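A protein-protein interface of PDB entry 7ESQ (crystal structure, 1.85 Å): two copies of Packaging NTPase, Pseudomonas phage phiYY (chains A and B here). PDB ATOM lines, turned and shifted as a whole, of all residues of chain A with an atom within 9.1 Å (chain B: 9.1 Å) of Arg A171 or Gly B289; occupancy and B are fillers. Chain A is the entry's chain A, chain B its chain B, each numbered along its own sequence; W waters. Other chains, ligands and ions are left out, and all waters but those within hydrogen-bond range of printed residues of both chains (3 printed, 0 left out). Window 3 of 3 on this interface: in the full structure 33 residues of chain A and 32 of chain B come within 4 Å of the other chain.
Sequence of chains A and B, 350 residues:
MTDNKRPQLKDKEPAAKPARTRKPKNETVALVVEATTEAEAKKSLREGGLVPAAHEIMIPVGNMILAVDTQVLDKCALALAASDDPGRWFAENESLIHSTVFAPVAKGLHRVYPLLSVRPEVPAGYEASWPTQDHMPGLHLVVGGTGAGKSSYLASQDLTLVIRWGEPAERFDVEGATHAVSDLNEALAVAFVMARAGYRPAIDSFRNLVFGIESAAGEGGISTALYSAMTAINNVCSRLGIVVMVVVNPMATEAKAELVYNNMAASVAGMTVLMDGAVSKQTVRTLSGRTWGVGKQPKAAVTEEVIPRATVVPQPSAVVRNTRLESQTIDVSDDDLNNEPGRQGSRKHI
Among the printed residues, merely in contact across the chains: Pro A168 with Arg B285 (3.7 Å), Ala A169 with Met B136 (3.7 Å), Ala A169 with Pro B120 (3.8 Å), Glu A170 with Met B136 (3.8 Å), Arg A164 with Pro B120 (3.8 Å), Asp A173 with Pro B120 (3.9 Å) and Arg A171 with Gly B289 (3.99 Å).
Of the 17 printed residues of chain B, 5 touch a printed residue of chain A. Printed residues of chain B that touch a printed residue of chain A: Pro B120, Met B136, Arg B285, Gly B289 and Arg B290. Hydrophobic or aromatic side chains of chain B that line the printed part of chain A: Pro B120 and Met B136. Along chain B the printed residues that touch a printed residue of chain A span positions 120 to 290. Hydrophobic or aromatic side chains of chain A that line the printed part of chain B: Pro A168. Along chain A the printed residues that touch a printed residue of chain B span positions 164 to 173. Among the printed residues, 9 pairs touch across the chains.
NH1 of Arg B285 is in salt-bridge range of OE1 of Glu A170. OE1 of Glu A170 lies within salt-bridge range of NH2 of Arg B290 (3.8 Å).
Water W1 bridges the backbone carbonyl oxygen (O) of Ala A169 (2.8 Å) and the backbone carbonyl oxygen (O) of Pro B137 (3.0 Å). Water W2 lies within hydrogen-bond range of O of Asp A173 (3.0 Å) and N of Val B122 (3.0 Å). Water W3 lies within hydrogen-bond range of the guanidinium group of Arg B285 (3.2 Å) and the side-chain carboxylate of Glu A170 (3.4 Å).
Of the printed residues of chain B, Glu A170 touches Met B136 (3.8 Å), Arg B285 (3.5 Å) and Arg B290 (3.8 Å). Printed residues of chain B within 4 Å of Arg A171: Gly B289. No residue of chain B comes within 4 Å of Phe A172. Val A174 touches none of the printed residues of chain B. No residue of chain B comes within 4 Å of Glu A175. Gln B133 touches none of the printed residues of chain A. Printed residues of chain A within 4 Å of Met B136: Ala A169 (3.7 Å) and Glu A170 (3.8 Å). No residue of chain A comes within 4 Å of Ser B288. The nearest printed residue of chain B that does not touch Arg A171 is Arg B290 (4.3 Å). The nearest printed residue of chain A that does not touch Gly B289 is Glu A175 (6.6 Å).
No position is printed for both chains. Of the 9 pairs that touch across the chains among the printed residues, none has its exchanged pair printed and touching as well.
The guanidinium group (NH2) of Arg A164 lies within hydrogen-bond range of the backbone carbonyl oxygen (O) of Pro A168, at 2.9 Å. The guanidinium group (NH2) of Arg A164 is in salt-bridge range of the side-chain carboxylate (OE2) of Glu A170 (2.8 Å). The side-chain carboxylate of Asp A173 is in salt-bridge range of the guanidinium group of Arg A164 (2.7 Å). N of Glu A170 sits at hydrogen-bond distance from OD2 of Asp A173, 2.7 Å away. The backbone NH of Arg B285 lies within hydrogen-bond range of the backbone carbonyl oxygen of Ala B269, 2.8 Å away. OG1 of Thr B286 sits at hydrogen-bond distance from N of Gly B289 (3.1 Å).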
ATOM      1  N   GLY A 147      -9.720  29.246 -10.757  1.00  0.00           N
ATOM      2  CA  GLY A 147      -9.495  27.864 -10.372  1.00  0.00           C
ATOM      3  C   GLY A 147      -9.334  26.888 -11.516  1.00  0.00           C
ATOM      4  O   GLY A 147      -9.530  25.686 -11.323  1.00  0.00           O
ATOM      5  N   GLY A 149      -6.655  25.902 -12.748  1.00  0.00           N
ATOM      6  CA  GLY A 149      -5.393  25.203 -12.617  1.00  0.00           C
ATOM      7  C   GLY A 149      -4.199  25.869 -13.274  1.00  0.00           C
ATOM      8  O   GLY A 149      -3.195  25.193 -13.519  1.00  0.00           O
ATOM      9  N   SER A 151      -2.077  28.274 -12.067  1.00  0.00           N
ATOM     10  CA  SER A 151      -0.897  28.349 -11.203  1.00  0.00           C
ATOM     11  C   SER A 151      -0.214  26.989 -11.059  1.00  0.00           C
ATOM     12  O   SER A 151       1.022  26.900 -11.062  1.00  0.00           O
ATOM     13  CB  SER A 151      -1.262  28.891  -9.818  1.00  0.00           C
ATOM     14  OG  SER A 151      -1.670  30.252  -9.852  1.00  0.00           O
ATOM     15  N   SER A 152      -0.992  25.920 -10.883  1.00  0.00           N
ATOM     16  CA  SER A 152      -0.338  24.618 -10.740  1.00  0.00           C
ATOM     17  C   SER A 152       0.196  24.104 -12.072  1.00  0.00           C
ATOM     18  O   SER A 152       1.157  23.328 -12.077  1.00  0.00           O
ATOM     19  CB  SER A 152      -1.291  23.595 -10.110  1.00  0.00           C
ATOM     20  OG  SER A 152      -2.342  23.311 -11.004  1.00  0.00           O
ATOM     21  N   TYR A 153      -0.375  24.540 -13.200  1.00  0.00           N
ATOM     22  CA  TYR A 153       0.149  24.128 -14.504  1.00  0.00           C
ATOM     23  C   TYR A 153       1.610  24.535 -14.675  1.00  0.00           C
ATOM     24  O   TYR A 153       2.398  23.804 -15.291  1.00  0.00           O
ATOM     25  CB  TYR A 153      -0.692  24.732 -15.623  1.00  0.00           C
ATOM     26  CG  TYR A 153      -0.191  24.459 -17.033  1.00  0.00           C
ATOM     27  CD1 TYR A 153      -0.448  23.240 -17.659  1.00  0.00           C
ATOM     28  CD2 TYR A 153       0.553  25.412 -17.734  1.00  0.00           C
ATOM     29  CE1 TYR A 153      -0.008  22.986 -18.952  1.00  0.00           C
ATOM     30  CE2 TYR A 153       1.006  25.159 -19.040  1.00  0.00           C
ATOM     31  CZ  TYR A 153       0.721  23.935 -19.635  1.00  0.00           C
ATOM     32  OH  TYR A 153       1.149  23.655 -20.919  1.00  0.00           O
ATOM     33  N   ARG A 164       5.742  35.992  -8.745  1.00  0.00           N
ATOM     34  CA  ARG A 164       4.387  36.091  -8.212  1.00  0.00           C
ATOM     35  C   ARG A 164       3.990  37.561  -8.082  1.00  0.00           C
ATOM     36  O   ARG A 164       4.669  38.337  -7.405  1.00  0.00           O
ATOM     37  CB  ARG A 164       4.294  35.368  -6.868  1.00  0.00           C
ATOM     38  CG  ARG A 164       4.465  33.846  -7.037  1.00  0.00           C
ATOM     39  CD  ARG A 164       3.126  33.199  -7.403  1.00  0.00           C
ATOM     40  NE  ARG A 164       2.225  33.236  -6.243  1.00  0.00           N
ATOM     41  CZ  ARG A 164       0.911  33.051  -6.311  1.00  0.00           C
ATOM     42  NH1 ARG A 164       0.329  32.809  -7.470  1.00  0.00           N
ATOM     43  NH2 ARG A 164       0.170  33.110  -5.212  1.00  0.00           N
ATOM     44  N   PRO A 168      -3.051  36.452  -4.348  1.00  0.00           N
ATOM     45  CA  PRO A 168      -2.980  36.284  -2.887  1.00  0.00           C
ATOM     46  C   PRO A 168      -1.920  35.274  -2.491  1.00  0.00           C
ATOM     47  O   PRO A 168      -1.600  34.357  -3.246  1.00  0.00           O
ATOM     48  CB  PRO A 168      -4.380  35.771  -2.521  1.00  0.00           C
ATOM     49  CG  PRO A 168      -4.801  34.986  -3.769  1.00  0.00           C
ATOM     50  CD  PRO A 168      -4.255  35.820  -4.924  1.00  0.00           C
ATOM     51  N   ALA A 169      -1.391  35.433  -1.278  1.00  0.00           N
ATOM     52  CA  ALA A 169      -0.414  34.483  -0.770  1.00  0.00           C
ATOM     53  C   ALA A 169      -1.045  33.099  -0.738  1.00  0.00           C
ATOM     54  O   ALA A 169      -2.159  32.923  -0.234  1.00  0.00           O
ATOM     55  CB  ALA A 169       0.064  34.885   0.626  1.00  0.00           C
ATOM     56  N   GLU A 170      -0.349  32.127  -1.315  1.00  0.00           N
ATOM     57  CA  GLU A 170      -0.864  30.776  -1.487  1.00  0.00           C
ATOM     58  C   GLU A 170       0.204  29.785  -1.058  1.00  0.00           C
ATOM     59  O   GLU A 170       1.319  30.164  -0.679  1.00  0.00           O
ATOM     60  CB  GLU A 170      -1.276  30.504  -2.944  1.00  0.00           C
ATOM     61  CG  GLU A 170      -2.606  31.147  -3.368  1.00  0.00           C
ATOM     62  CD  GLU A 170      -2.810  31.136  -4.885  1.00  0.00           C
ATOM     63  OE1 GLU A 170      -3.396  30.149  -5.385  1.00  0.00           O
ATOM     64  OE2 GLU A 170      -2.435  32.124  -5.576  1.00  0.00           O
ATOM     65  N   ARG A 171      -0.136  28.495  -1.149  1.00  0.00           N
ATOM     66  CA  ARG A 171       0.863  27.461  -0.904  1.00  0.00           C
ATOM     67  C   ARG A 171       2.069  27.626  -1.829  1.00  0.00           C
ATOM     68  O   ARG A 171       3.201  27.359  -1.419  1.00  0.00           O
ATOM     69  CB  ARG A 171       0.231  26.071  -1.066  1.00  0.00           C
ATOM     70  CG  ARG A 171      -0.047  25.658  -2.526  1.00  0.00           C
ATOM     71  CD  ARG A 171      -0.614  24.233  -2.656  1.00  0.00           C
ATOM     72  NE  ARG A 171      -1.403  24.057  -3.878  1.00  0.00           N
ATOM     73  CZ  ARG A 171      -2.727  23.911  -3.915  1.00  0.00           C
ATOM     74  NH1 ARG A 171      -3.439  23.916  -2.790  1.00  0.00           N
ATOM     75  NH2 ARG A 171      -3.344  23.759  -5.083  1.00  0.00           N
ATOM     76  N   PHE A 172       1.852  28.111  -3.059  1.00  0.00           N
ATOM     77  CA  PHE A 172       2.958  28.292  -4.001  1.00  0.00           C
ATOM     78  C   PHE A 172       4.049  29.201  -3.436  1.00  0.00           C
ATOM     79  O   PHE A 172       5.231  29.023  -3.757  1.00  0.00           O
ATOM     80  CB  PHE A 172       2.441  28.869  -5.325  1.00  0.00           C
ATOM     81  CG  PHE A 172       1.248  28.136  -5.893  1.00  0.00           C
ATOM     82  CD1 PHE A 172       1.383  26.859  -6.423  1.00  0.00           C
ATOM     83  CD2 PHE A 172      -0.008  28.727  -5.894  1.00  0.00           C
ATOM     84  CE1 PHE A 172       0.291  26.178  -6.937  1.00  0.00           C
ATOM     85  CE2 PHE A 172      -1.111  28.046  -6.404  1.00  0.00           C
ATOM     86  CZ  PHE A 172      -0.955  26.770  -6.930  1.00  0.00           C
ATOM     87  N   ASP A 173       3.684  30.164  -2.589  1.00  0.00           N
ATOM     88  CA  ASP A 173       4.620  31.201  -2.175  1.00  0.00           C
ATOM     89  C   ASP A 173       5.511  30.807  -1.017  1.00  0.00           C
ATOM     90  O   ASP A 173       6.471  31.525  -0.732  1.00  0.00           O
ATOM     91  CB  ASP A 173       3.871  32.462  -1.784  1.00  0.00           C
ATOM     92  CG  ASP A 173       3.023  32.971  -2.901  1.00  0.00           C
ATOM     93  OD1 ASP A 173       3.610  33.437  -3.906  1.00  0.00           O
ATOM     94  OD2 ASP A 173       1.786  32.891  -2.778  1.00  0.00           O
ATOM     95  N   VAL A 174       5.209  29.725  -0.312  1.00  0.00           N
ATOM     96  CA  VAL A 174       6.052  29.291   0.784  1.00  0.00           C
ATOM     97  C   VAL A 174       6.856  28.053   0.419  1.00  0.00           C
ATOM     98  O   VAL A 174       8.004  27.918   0.861  1.00  0.00           O
ATOM     99  CB  VAL A 174       5.209  29.054   2.054  1.00  0.00           C
ATOM    100  CG1 VAL A 174       4.344  27.828   1.893  1.00  0.00           C
ATOM    101  CG2 VAL A 174       6.101  28.940   3.282  1.00  0.00           C
ATOM    102  N   GLU A 175       6.321  27.196  -0.439  1.00  0.00           N
ATOM    103  CA  GLU A 175       6.965  25.979  -0.912  1.00  0.00           C
ATOM    104  C   GLU A 175       7.213  26.168  -2.410  1.00  0.00           C
ATOM    105  O   GLU A 175       6.308  26.010  -3.234  1.00  0.00           O
ATOM    106  CB  GLU A 175       6.083  24.759  -0.596  1.00  0.00           C
ATOM    107  CG  GLU A 175       4.744  24.742  -1.363  1.00  0.00           C
ATOM    108  CD  GLU A 175       3.815  23.600  -1.037  1.00  0.00           C
ATOM    109  OE1 GLU A 175       4.143  22.782  -0.151  1.00  0.00           O
ATOM    110  OE2 GLU A 175       2.762  23.506  -1.715  1.00  0.00           O
ATOM    111  N   GLY A 176       8.416  26.541  -2.793  1.00  0.00           N
ATOM    112  CA  GLY A 176       8.711  26.545  -4.213  1.00  0.00           C
ATOM    113  C   GLY A 176       9.619  27.690  -4.597  1.00  0.00           C
ATOM    114  O   GLY A 176       9.885  28.605  -3.820  1.00  0.00           O
ATOM    115  N   ALA A 177      10.099  27.610  -5.835  1.00  0.00           N
ATOM    116  CA  ALA A 177      10.982  28.626  -6.404  1.00  0.00           C
ATOM    117  C   ALA A 177      10.099  29.747  -6.939  1.00  0.00           C
ATOM    118  O   ALA A 177       9.605  29.701  -8.067  1.00  0.00           O
ATOM    119  CB  ALA A 177      11.866  28.024  -7.491  1.00  0.00           C
ATOM    120  N   THR A 178       9.867  30.750  -6.101  1.00  0.00           N
ATOM    121  CA  THR A 178       9.135  31.943  -6.504  1.00  0.00           C
ATOM    122  C   THR A 178       9.925  33.179  -6.107  1.00  0.00           C
ATOM    123  O   THR A 178      10.811  33.135  -5.252  1.00  0.00           O
ATOM    124  CB  THR A 178       7.735  32.012  -5.874  1.00  0.00           C
ATOM    125  OG1 THR A 178       7.853  32.104  -4.451  1.00  0.00           O
ATOM    126  CG2 THR A 178       6.894  30.798  -6.237  1.00  0.00           C
ATOM    127  N   PRO B 120       3.008  38.886  -2.339  1.00  0.00           N
ATOM    128  CA  PRO B 120       2.531  37.729  -1.556  1.00  0.00           C
ATOM    129  C   PRO B 120       3.693  37.081  -0.814  1.00  0.00           C
ATOM    130  O   PRO B 120       4.573  36.466  -1.425  1.00  0.00           O
ATOM    131  CB  PRO B 120       1.952  36.792  -2.630  1.00  0.00           C
ATOM    132  CG  PRO B 120       2.652  37.184  -3.899  1.00  0.00           C
ATOM    133  CD  PRO B 120       2.846  38.684  -3.784  1.00  0.00           C
ATOM    134  N   VAL B 122       4.811  34.894   3.076  1.00  0.00           N
ATOM    135  CA  VAL B 122       4.470  34.271   4.348  1.00  0.00           C
ATOM    136  C   VAL B 122       5.730  34.310   5.201  1.00  0.00           C
ATOM    137  O   VAL B 122       6.756  33.746   4.808  1.00  0.00           O
ATOM    138  CB  VAL B 122       3.977  32.824   4.186  1.00  0.00           C
ATOM    139  CG1 VAL B 122       3.595  32.204   5.549  1.00  0.00           C
ATOM    140  CG2 VAL B 122       2.788  32.788   3.261  1.00  0.00           C
ATOM    141  N   GLN B 133      -7.251  26.009  11.986  1.00  0.00           N
ATOM    142  CA  GLN B 133      -5.900  25.488  12.136  1.00  0.00           C
ATOM    143  C   GLN B 133      -5.135  25.631  10.827  1.00  0.00           C
ATOM    144  O   GLN B 133      -5.636  25.256   9.765  1.00  0.00           O
ATOM    145  CB  GLN B 133      -5.945  24.022  12.584  1.00  0.00           C
ATOM    146  CG  GLN B 133      -4.592  23.451  12.974  1.00  0.00           C
ATOM    147  CD  GLN B 133      -3.964  24.155  14.169  1.00  0.00           C
ATOM    148  OE1 GLN B 133      -4.626  24.429  15.178  1.00  0.00           O
ATOM    149  NE2 GLN B 133      -2.671  24.455  14.058  1.00  0.00           N
ATOM    150  N   ASP B 134      -3.928  26.200  10.908  1.00  0.00           N
ATOM    151  CA  ASP B 134      -3.019  26.385   9.769  1.00  0.00           C
ATOM    152  C   ASP B 134      -3.586  27.310   8.687  1.00  0.00           C
ATOM    153  O   ASP B 134      -3.194  27.214   7.522  1.00  0.00           O
ATOM    154  CB  ASP B 134      -2.613  25.043   9.146  1.00  0.00           C
ATOM    155  CG  ASP B 134      -2.094  24.049  10.178  1.00  0.00           C
ATOM    156  OD1 ASP B 134      -1.468  24.481  11.177  1.00  0.00           O
ATOM    157  OD2 ASP B 134      -2.311  22.833   9.979  1.00  0.00           O
ATOM    158  N   HIS B 135      -4.504  28.200   9.058  1.00  0.00           N
ATOM    159  CA  HIS B 135      -5.033  29.216   8.149  1.00  0.00           C
ATOM    160  C   HIS B 135      -3.894  30.063   7.566  1.00  0.00           C
ATOM    161  O   HIS B 135      -3.061  30.575   8.316  1.00  0.00           O
ATOM    162  CB  HIS B 135      -6.026  30.079   8.950  1.00  0.00           C
ATOM    163  CG  HIS B 135      -6.994  30.877   8.127  1.00  0.00           C
ATOM    164  ND1 HIS B 135      -6.595  31.852   7.241  1.00  0.00           N
ATOM    165  CD2 HIS B 135      -8.349  30.879   8.104  1.00  0.00           C
ATOM    166  CE1 HIS B 135      -7.662  32.400   6.680  1.00  0.00           C
ATOM    167  NE2 HIS B 135      -8.740  31.830   7.191  1.00  0.00           N
ATOM    168  N   MET B 136      -3.831  30.178   6.225  1.00  0.00           N
ATOM    169  CA  MET B 136      -2.921  31.137   5.585  1.00  0.00           C
ATOM    170  C   MET B 136      -3.100  32.527   6.189  1.00  0.00           C
ATOM    171  O   MET B 136      -4.236  32.939   6.460  1.00  0.00           O
ATOM    172  CB  MET B 136      -3.176  31.206   4.068  1.00  0.00           C
ATOM    173  CG  MET B 136      -2.654  30.082   3.161  1.00  0.00           C
ATOM    174  SD  MET B 136      -0.862  29.794   3.225  1.00  0.00           S
ATOM    175  CE  MET B 136      -0.276  31.350   2.595  1.00  0.00           C
ATOM    176  N   PRO B 137      -2.022  33.281   6.408  1.00  0.00           N
ATOM    177  CA  PRO B 137      -2.200  34.690   6.770  1.00  0.00           C
ATOM    178  C   PRO B 137      -2.854  35.431   5.613  1.00  0.00           C
ATOM    179  O   PRO B 137      -2.615  35.128   4.442  1.00  0.00           O
ATOM    180  CB  PRO B 137      -0.770  35.181   7.038  1.00  0.00           C
ATOM    181  CG  PRO B 137       0.085  34.333   6.121  1.00  0.00           C
ATOM    182  CD  PRO B 137      -0.604  32.951   6.155  1.00  0.00           C
ATOM    183  N   ALA B 269      -7.289  34.580   1.684  1.00  0.00           N
ATOM    184  CA  ALA B 269      -6.891  33.347   2.364  1.00  0.00           C
ATOM    185  C   ALA B 269      -8.087  32.463   2.721  1.00  0.00           C
ATOM    186  O   ALA B 269      -7.986  31.230   2.659  1.00  0.00           O
ATOM    187  CB  ALA B 269      -6.115  33.683   3.641  1.00  0.00           C
ATOM    188  N   THR B 283     -14.379  28.028   3.011  1.00  0.00           N
ATOM    189  CA  THR B 283     -13.187  27.540   2.335  1.00  0.00           C
ATOM    190  C   THR B 283     -11.990  28.333   2.839  1.00  0.00           C
ATOM    191  O   THR B 283     -12.069  29.561   2.984  1.00  0.00           O
ATOM    192  CB  THR B 283     -13.337  27.637   0.808  1.00  0.00           C
ATOM    193  OG1 THR B 283     -12.138  27.185   0.164  1.00  0.00           O
ATOM    194  CG2 THR B 283     -13.653  29.050   0.374  1.00  0.00           C
ATOM    195  N   VAL B 284     -10.907  27.621   3.156  1.00  0.00           N
ATOM    196  CA  VAL B 284      -9.715  28.201   3.771  1.00  0.00           C
ATOM    197  C   VAL B 284      -8.480  27.609   3.105  1.00  0.00           C
ATOM    198  O   VAL B 284      -8.340  26.385   3.022  1.00  0.00           O
ATOM    199  CB  VAL B 284      -9.667  27.943   5.291  1.00  0.00           C
ATOM    200  CG1 VAL B 284      -8.313  28.359   5.865  1.00  0.00           C
ATOM    201  CG2 VAL B 284     -10.790  28.679   6.002  1.00  0.00           C
ATOM    202  N   ARG B 285      -7.583  28.474   2.633  1.00  0.00           N
ATOM    203  CA  ARG B 285      -6.268  28.028   2.187  1.00  0.00           C
ATOM    204  C   ARG B 285      -5.417  27.774   3.422  1.00  0.00           C
ATOM    205  O   ARG B 285      -5.315  28.639   4.295  1.00  0.00           O
ATOM    206  CB  ARG B 285      -5.589  29.085   1.319  1.00  0.00           C
ATOM    207  CG  ARG B 285      -6.306  29.447   0.047  1.00  0.00           C
ATOM    208  CD  ARG B 285      -5.447  30.413  -0.747  1.00  0.00           C
ATOM    209  NE  ARG B 285      -6.261  31.433  -1.391  1.00  0.00           N
ATOM    210  CZ  ARG B 285      -6.640  31.406  -2.663  1.00  0.00           C
ATOM    211  NH1 ARG B 285      -6.300  30.394  -3.443  1.00  0.00           N
ATOM    212  NH2 ARG B 285      -7.383  32.381  -3.142  1.00  0.00           N
ATOM    213  N   THR B 286      -4.807  26.601   3.503  1.00  0.00           N
ATOM    214  CA  THR B 286      -3.988  26.267   4.657  1.00  0.00           C
ATOM    215  C   THR B 286      -2.536  26.098   4.235  1.00  0.00           C
ATOM    216  O   THR B 286      -2.230  25.835   3.069  1.00  0.00           O
ATOM    217  CB  THR B 286      -4.476  24.989   5.359  1.00  0.00           C
ATOM    218  OG1 THR B 286      -4.459  23.896   4.432  1.00  0.00           O
ATOM    219  CG2 THR B 286      -5.888  25.170   5.879  1.00  0.00           C
ATOM    220  N   LEU B 287      -1.647  26.249   5.222  1.00  0.00           N
ATOM    221  CA  LEU B 287      -0.214  26.083   4.993  1.00  0.00           C
ATOM    222  C   LEU B 287       0.100  24.760   4.308  1.00  0.00           C
ATOM    223  O   LEU B 287       1.033  24.677   3.498  1.00  0.00           O
ATOM    224  CB  LEU B 287       0.519  26.195   6.326  1.00  0.00           C
ATOM    225  CG  LEU B 287       0.393  27.617   6.851  1.00  0.00           C
ATOM    226  CD1 LEU B 287       0.947  27.735   8.249  1.00  0.00           C
ATOM    227  CD2 LEU B 287       1.189  28.486   5.907  1.00  0.00           C
ATOM    228  N   SER B 288      -0.678  23.719   4.602  1.00  0.00           N
ATOM    229  CA  SER B 288      -0.524  22.461   3.885  1.00  0.00           C
ATOM    230  C   SER B 288      -1.847  22.025   3.246  1.00  0.00           C
ATOM    231  O   SER B 288      -2.378  20.960   3.583  1.00  0.00           O
ATOM    232  CB  SER B 288       0.024  21.386   4.829  1.00  0.00           C
ATOM    233  OG  SER B 288       0.118  20.123   4.189  1.00  0.00           O
ATOM    234  N   GLY B 289      -2.394  22.836   2.342  1.00  0.00           N
ATOM    235  CA  GLY B 289      -3.544  22.415   1.541  1.00  0.00           C
ATOM    236  C   GLY B 289      -4.497  23.571   1.238  1.00  0.00           C
ATOM    237  O   GLY B 289      -4.076  24.718   1.069  1.00  0.00           O
ATOM    238  N   ARG B 290      -5.779  23.210   1.126  1.00  0.00           N
ATOM    239  CA  ARG B 290      -6.878  24.153   0.914  1.00  0.00           C
ATOM    240  C   ARG B 290      -8.143  23.451   1.387  1.00  0.00           C
ATOM    241  O   ARG B 290      -8.526  22.428   0.808  1.00  0.00           O
ATOM    242  CB  ARG B 290      -7.035  24.548  -0.568  1.00  0.00           C
ATOM    243  CG  ARG B 290      -8.135  25.607  -0.791  1.00  0.00           C
ATOM    244  CD  ARG B 290      -8.358  26.063  -2.256  1.00  0.00           C
ATOM    245  NE  ARG B 290      -7.273  26.795  -2.918  1.00  0.00           N
ATOM    246  CZ  ARG B 290      -7.283  27.101  -4.218  1.00  0.00           C
ATOM    247  NH1 ARG B 290      -8.335  26.783  -4.965  1.00  0.00           N
ATOM    248  NH2 ARG B 290      -6.262  27.749  -4.770  1.00  0.00           N
ATOM    249  N   THR B 291      -8.795  23.983   2.417  1.00  0.00           N
ATOM    250  CA  THR B 291     -10.039  23.385   2.914  1.00  0.00           C
ATOM    251  C   THR B 291     -11.241  24.305   2.683  1.00  0.00           C
ATOM    252  O   THR B 291     -11.528  24.710   1.550  1.00  0.00           O
ATOM    253  CB  THR B 291      -9.954  23.055   4.419  1.00  0.00           C
ATOM    254  OG1 THR B 291      -9.744  24.261   5.162  1.00  0.00           O
ATOM    255  CG2 THR B 291      -8.803  22.102   4.696  1.00  0.00           C
HETATM  256  O   HOH W   1      -3.448  34.668   1.578  1.00  0.00           O
HETATM  257  O   HOH W   2       6.925  33.821   1.176  1.00  0.00           O
HETATM  258  O   HOH W   3      -6.231  31.853  -6.297  1.00  0.00           O
